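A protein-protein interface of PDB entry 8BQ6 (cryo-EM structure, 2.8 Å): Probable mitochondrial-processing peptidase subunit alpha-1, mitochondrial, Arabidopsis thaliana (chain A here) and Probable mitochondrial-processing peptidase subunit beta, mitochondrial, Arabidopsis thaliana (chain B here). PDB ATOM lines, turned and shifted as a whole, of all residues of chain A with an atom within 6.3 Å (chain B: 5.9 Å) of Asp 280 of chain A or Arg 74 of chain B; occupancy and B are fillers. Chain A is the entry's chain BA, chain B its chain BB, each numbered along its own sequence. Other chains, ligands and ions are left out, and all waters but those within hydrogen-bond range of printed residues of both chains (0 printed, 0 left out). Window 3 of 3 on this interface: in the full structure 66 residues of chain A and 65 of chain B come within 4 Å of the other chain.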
ATOM      1  N   ASN A  85      -9.556   7.107  32.991  1.00  0.00           N
ATOM      2  CA  ASN A  85      -8.352   7.921  33.062  1.00  0.00           C
ATOM      3  C   ASN A  85      -8.040   8.393  34.477  1.00  0.00           C
ATOM      4  O   ASN A  85      -6.969   8.968  34.697  1.00  0.00           O
ATOM      5  CB  ASN A  85      -8.449   9.127  32.118  1.00  0.00           C
ATOM      6  CG  ASN A  85      -9.735   9.918  32.287  1.00  0.00           C
ATOM      7  OD1 ASN A  85     -10.252  10.069  33.393  1.00  0.00           O
ATOM      8  ND2 ASN A  85     -10.235  10.463  31.185  1.00  0.00           N
ATOM      9  N   GLU A 175     -20.534  22.242  29.938  1.00  0.00           N
ATOM     10  CA  GLU A 175     -19.850  22.430  28.664  1.00  0.00           C
ATOM     11  C   GLU A 175     -18.906  23.624  28.711  1.00  0.00           C
ATOM     12  O   GLU A 175     -17.760  23.545  28.257  1.00  0.00           O
ATOM     13  CB  GLU A 175     -20.880  22.612  27.558  1.00  0.00           C
ATOM     14  CG  GLU A 175     -20.288  23.015  26.243  1.00  0.00           C
ATOM     15  CD  GLU A 175     -21.348  23.298  25.216  1.00  0.00           C
ATOM     16  OE1 GLU A 175     -22.042  22.348  24.805  1.00  0.00           O
ATOM     17  OE2 GLU A 175     -21.478  24.470  24.810  1.00  0.00           O
ATOM     18  N   ARG A 182     -10.062  22.725  29.851  1.00  0.00           N
ATOM     19  CA  ARG A 182      -9.399  21.735  29.013  1.00  0.00           C
ATOM     20  C   ARG A 182      -8.714  22.365  27.807  1.00  0.00           C
ATOM     21  O   ARG A 182      -7.633  21.919  27.408  1.00  0.00           O
ATOM     22  CB  ARG A 182     -10.405  20.680  28.555  1.00  0.00           C
ATOM     23  CG  ARG A 182     -10.656  19.600  29.584  1.00  0.00           C
ATOM     24  CD  ARG A 182     -10.758  18.232  28.940  1.00  0.00           C
ATOM     25  NE  ARG A 182      -9.897  18.110  27.772  1.00  0.00           N
ATOM     26  CZ  ARG A 182     -10.002  17.148  26.866  1.00  0.00           C
ATOM     27  NH1 ARG A 182     -10.932  16.213  26.958  1.00  0.00           N
ATOM     28  NH2 ARG A 182      -9.150  17.122  25.846  1.00  0.00           N
ATOM     29  N   ASN A 183      -9.308  23.400  27.214  1.00  0.00           N
ATOM     30  CA  ASN A 183      -8.825  23.964  25.953  1.00  0.00           C
ATOM     31  C   ASN A 183      -8.637  25.479  26.006  1.00  0.00           C
ATOM     32  O   ASN A 183      -9.247  26.209  25.221  1.00  0.00           O
ATOM     33  CB  ASN A 183      -9.787  23.605  24.825  1.00  0.00           C
ATOM     34  CG  ASN A 183     -10.290  22.187  24.918  1.00  0.00           C
ATOM     35  OD1 ASN A 183      -9.505  21.243  24.963  1.00  0.00           O
ATOM     36  ND2 ASN A 183     -11.607  22.026  24.951  1.00  0.00           N
ATOM     37  N   GLU A 275     -19.019  12.940  30.490  1.00  0.00           N
ATOM     38  CA  GLU A 275     -18.186  11.842  29.998  1.00  0.00           C
ATOM     39  C   GLU A 275     -17.634  12.084  28.597  1.00  0.00           C
ATOM     40  O   GLU A 275     -16.419  11.907  28.402  1.00  0.00           O
ATOM     41  CB  GLU A 275     -18.964  10.526  30.073  1.00  0.00           C
ATOM     42  CG  GLU A 275     -18.409   9.546  31.084  1.00  0.00           C
ATOM     43  CD  GLU A 275     -19.466   8.599  31.606  1.00  0.00           C
ATOM     44  OE1 GLU A 275     -19.269   8.035  32.701  1.00  0.00           O
ATOM     45  OE2 GLU A 275     -20.494   8.421  30.921  1.00  0.00           O
ATOM     46  N   PRO A 276     -18.428  12.479  27.594  1.00  0.00           N
ATOM     47  CA  PRO A 276     -17.841  12.734  26.266  1.00  0.00           C
ATOM     48  C   PRO A 276     -16.832  13.867  26.239  1.00  0.00           C
ATOM     49  O   PRO A 276     -16.028  13.929  25.303  1.00  0.00           O
ATOM     50  CB  PRO A 276     -19.065  13.061  25.398  1.00  0.00           C
ATOM     51  CG  PRO A 276     -20.203  12.438  26.103  1.00  0.00           C
ATOM     52  CD  PRO A 276     -19.897  12.599  27.553  1.00  0.00           C
ATOM     53  N   LEU A 277     -16.853  14.775  27.213  1.00  0.00           N
ATOM     54  CA  LEU A 277     -15.909  15.884  27.232  1.00  0.00           C
ATOM     55  C   LEU A 277     -14.646  15.594  28.029  1.00  0.00           C
ATOM     56  O   LEU A 277     -13.720  16.411  28.002  1.00  0.00           O
ATOM     57  CB  LEU A 277     -16.567  17.144  27.805  1.00  0.00           C
ATOM     58  CG  LEU A 277     -17.869  17.644  27.186  1.00  0.00           C
ATOM     59  CD1 LEU A 277     -18.274  18.940  27.862  1.00  0.00           C
ATOM     60  CD2 LEU A 277     -17.733  17.830  25.684  1.00  0.00           C
ATOM     61  N   THR A 278     -14.584  14.467  28.736  1.00  0.00           N
ATOM     62  CA  THR A 278     -13.474  14.184  29.637  1.00  0.00           C
ATOM     63  C   THR A 278     -12.902  12.784  29.493  1.00  0.00           C
ATOM     64  O   THR A 278     -11.813  12.530  30.020  1.00  0.00           O
ATOM     65  CB  THR A 278     -13.904  14.372  31.099  1.00  0.00           C
ATOM     66  OG1 THR A 278     -15.137  13.678  31.325  1.00  0.00           O
ATOM     67  CG2 THR A 278     -14.089  15.847  31.425  1.00  0.00           C
ATOM     68  N   SER A 279     -13.596  11.870  28.813  1.00  0.00           N
ATOM     69  CA  SER A 279     -13.141  10.488  28.724  1.00  0.00           C
ATOM     70  C   SER A 279     -11.862  10.338  27.916  1.00  0.00           C
ATOM     71  O   SER A 279     -11.139   9.354  28.103  1.00  0.00           O
ATOM     72  CB  SER A 279     -14.235   9.618  28.109  1.00  0.00           C
ATOM     73  OG  SER A 279     -14.478   9.993  26.763  1.00  0.00           O
ATOM     74  N   ASP A 280     -11.566  11.278  27.025  1.00  0.00           N
ATOM     75  CA  ASP A 280     -10.422  11.158  26.135  1.00  0.00           C
ATOM     76  C   ASP A 280      -9.143  11.736  26.723  1.00  0.00           C
ATOM     77  O   ASP A 280      -8.113  11.745  26.041  1.00  0.00           O
ATOM     78  CB  ASP A 280     -10.735  11.826  24.793  1.00  0.00           C
ATOM     79  CG  ASP A 280     -11.935  11.202  24.108  1.00  0.00           C
ATOM     80  OD1 ASP A 280     -12.303  11.650  23.003  1.00  0.00           O
ATOM     81  OD2 ASP A 280     -12.511  10.256  24.685  1.00  0.00           O
ATOM     82  N   LEU A 281      -9.178  12.209  27.957  1.00  0.00           N
ATOM     83  CA  LEU A 281      -7.958  12.667  28.608  1.00  0.00           C
ATOM     84  C   LEU A 281      -7.019  11.486  28.824  1.00  0.00           C
ATOM     85  O   LEU A 281      -7.469  10.409  29.233  1.00  0.00           O
ATOM     86  CB  LEU A 281      -8.286  13.333  29.936  1.00  0.00           C
ATOM     87  CG  LEU A 281      -8.849  14.749  29.854  1.00  0.00           C
ATOM     88  CD1 LEU A 281      -9.679  15.038  31.083  1.00  0.00           C
ATOM     89  CD2 LEU A 281      -7.730  15.761  29.718  1.00  0.00           C
ATOM     90  N   PRO A 282      -5.724  11.637  28.556  1.00  0.00           N
ATOM     91  CA  PRO A 282      -4.800  10.514  28.744  1.00  0.00           C
ATOM     92  C   PRO A 282      -4.663  10.139  30.212  1.00  0.00           C
ATOM     93  O   PRO A 282      -4.688  10.994  31.099  1.00  0.00           O
ATOM     94  CB  PRO A 282      -3.479  11.045  28.181  1.00  0.00           C
ATOM     95  CG  PRO A 282      -3.593  12.522  28.290  1.00  0.00           C
ATOM     96  CD  PRO A 282      -5.037  12.844  28.069  1.00  0.00           C
ATOM     97  N   ASP B  72     -13.782  22.276  17.830  1.00  0.00           N
ATOM     98  CA  ASP B  72     -14.332  20.948  18.060  1.00  0.00           C
ATOM     99  C   ASP B  72     -15.772  21.100  18.534  1.00  0.00           C
ATOM    100  O   ASP B  72     -16.024  21.695  19.588  1.00  0.00           O
ATOM    101  CB  ASP B  72     -13.485  20.186  19.079  1.00  0.00           C
ATOM    102  CG  ASP B  72     -13.983  18.767  19.316  1.00  0.00           C
ATOM    103  OD1 ASP B  72     -14.775  18.257  18.496  1.00  0.00           O
ATOM    104  OD2 ASP B  72     -13.562  18.149  20.315  1.00  0.00           O
ATOM    105  N   LYS B  73     -16.715  20.572  17.749  1.00  0.00           N
ATOM    106  CA  LYS B  73     -18.134  20.770  18.019  1.00  0.00           C
ATOM    107  C   LYS B  73     -18.625  19.984  19.225  1.00  0.00           C
ATOM    108  O   LYS B  73     -19.775  20.169  19.634  1.00  0.00           O
ATOM    109  CB  LYS B  73     -18.960  20.389  16.792  1.00  0.00           C
ATOM    110  CG  LYS B  73     -18.936  21.428  15.693  1.00  0.00           C
ATOM    111  CD  LYS B  73     -20.281  22.102  15.530  1.00  0.00           C
ATOM    112  CE  LYS B  73     -20.131  23.392  14.751  1.00  0.00           C
ATOM    113  NZ  LYS B  73     -19.300  24.382  15.488  1.00  0.00           N
ATOM    114  N   ARG B  74     -17.793  19.101  19.779  1.00  0.00           N
ATOM    115  CA  ARG B  74     -18.134  18.437  21.031  1.00  0.00           C
ATOM    116  C   ARG B  74     -18.474  19.453  22.112  1.00  0.00           C
ATOM    117  O   ARG B  74     -19.355  19.216  22.946  1.00  0.00           O
ATOM    118  CB  ARG B  74     -16.967  17.561  21.486  1.00  0.00           C
ATOM    119  CG  ARG B  74     -16.942  16.165  20.911  1.00  0.00           C
ATOM    120  CD  ARG B  74     -15.908  15.324  21.640  1.00  0.00           C
ATOM    121  NE  ARG B  74     -14.581  15.926  21.589  1.00  0.00           N
ATOM    122  CZ  ARG B  74     -13.675  15.831  22.554  1.00  0.00           C
ATOM    123  NH1 ARG B  74     -13.929  15.182  23.678  1.00  0.00           N
ATOM    124  NH2 ARG B  74     -12.485  16.400  22.386  1.00  0.00           N
ATOM    125  N   PHE B  75     -17.792  20.597  22.105  1.00  0.00           N
ATOM    126  CA  PHE B  75     -17.955  21.625  23.122  1.00  0.00           C
ATOM    127  C   PHE B  75     -18.889  22.748  22.699  1.00  0.00           C
ATOM    128  O   PHE B  75     -18.949  23.774  23.383  1.00  0.00           O
ATOM    129  CB  PHE B  75     -16.596  22.214  23.494  1.00  0.00           C
ATOM    130  CG  PHE B  75     -15.638  21.210  24.038  1.00  0.00           C
ATOM    131  CD1 PHE B  75     -14.796  20.508  23.194  1.00  0.00           C
ATOM    132  CD2 PHE B  75     -15.583  20.958  25.395  1.00  0.00           C
ATOM    133  CE1 PHE B  75     -13.914  19.576  23.696  1.00  0.00           C
ATOM    134  CE2 PHE B  75     -14.705  20.025  25.902  1.00  0.00           C
ATOM    135  CZ  PHE B  75     -13.868  19.334  25.052  1.00  0.00           C
ATOM    136  N   LEU B  76     -19.615  22.587  21.598  1.00  0.00           N
ATOM    137  CA  LEU B  76     -20.444  23.656  21.047  1.00  0.00           C
ATOM    138  C   LEU B  76     -21.836  23.138  20.708  1.00  0.00           C
ATOM    139  O   LEU B  76     -22.326  23.293  19.590  1.00  0.00           O
ATOM    140  CB  LEU B  76     -19.796  24.289  19.818  1.00  0.00           C
ATOM    141  CG  LEU B  76     -18.538  25.114  20.068  1.00  0.00           C
ATOM    142  CD1 LEU B  76     -18.031  25.706  18.774  1.00  0.00           C
ATOM    143  CD2 LEU B  76     -18.851  26.204  21.061  1.00  0.00           C
ATOM    144  N   LYS B  77     -22.486  22.486  21.668  1.00  0.00           N
ATOM    145  CA  LYS B  77     -23.799  21.914  21.421  1.00  0.00           C
ATOM    146  C   LYS B  77     -24.868  22.318  22.422  1.00  0.00           C
ATOM    147  O   LYS B  77     -26.055  22.167  22.115  1.00  0.00           O
ATOM    148  CB  LYS B  77     -23.711  20.384  21.395  1.00  0.00           C
ATOM    149  CG  LYS B  77     -23.268  19.792  22.711  1.00  0.00           C
ATOM    150  CD  LYS B  77     -23.076  18.294  22.603  1.00  0.00           C
ATOM    151  CE  LYS B  77     -24.299  17.620  22.000  1.00  0.00           C
ATOM    152  NZ  LYS B  77     -25.568  18.068  22.633  1.00  0.00           N
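The side-chain carboxylate (OE1) of Glu 175 of chain A is in hydrogen-bond range of the backbone NH (N) of Lys 77 of chain B, 3.2 Å away. The backbone carbonyl oxygen (O) of Pro 276 of chain A is in hydrogen-bond range of the guanidinium group (NH1) of Arg 74 of chain B (2.9 Å). The guanidinium group (NH1) of Arg 74 of chain B lies within salt-bridge range of the side-chain carboxylate (OD1) of Asp 280 of chain A. OE2 of Glu 175 of chain A sits close to O of Phe 75 of chain B (3.0 Å).
NH1 of Arg 182 of chain A lies within hydrogen-bond range of O of Leu 277 of chain A. The side-chain hydroxyl (OG) of Ser 279 of chain A sits at hydrogen-bond distance from the side-chain carboxylate (OD2) of Asp 280 of chain A, 2.9 Å away. The guanidinium group (NE) of Arg 74 of chain B is in salt-bridge range of the side-chain carboxylate (OD2) of Asp 72 of chain B.
CA of Leu 76 of chain B touches OE2 of Glu 175 of chain A, 3.99 Å away. Phe 75 of chain B touches Asn 183 of chain A. Leu 277 of chain A touches Arg 74 of chain B (CD2 to O, 3.5 Å). Phe 75 of chain B touches Leu 277 of chain A.
Of chain B, only Arg 74 (3.9 Å) comes within 4 Å of Asp 280 of chain A. Of the printed residues of chain A, Arg 74 of chain B touches Pro 276 (2.9 Å), Leu 277 (3.5 Å) and Asp 280 (3.9 Å). Of the printed residues of chain A, Leu 76 of chain B touches Glu 175. Of the printed residues of chain B, Pro 276 of chain A touches Arg 74. The nearest printed residue of chain B that does not touch Asp 280 of chain A is Asp 72 of chain B (7.1 Å). The nearest residue of chain A that does not touch Arg 74 of chain B is Glu 175 of chain A (4.5 Å). The nearest printed residue of chain A that does not touch Phe 75 of chain B is Arg 182 of chain A (4.7 Å).
Of the 6 printed residues of chain B, 4 touch a printed residue of chain A. Along chain B the printed residues that touch a printed residue of chain A span positions 74 to 77. Of the 12 printed residues of chain A, 5 touch a printed residue of chain B. Among the printed residues, 8 pairs touch across the chains. Among the printed residues, Asp or Glu carboxylates within 4 Å of a Lys or Arg side-chain nitrogen of the other chain: Asp 280 of chain A with Arg 74 of chain B (3.9 Å).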
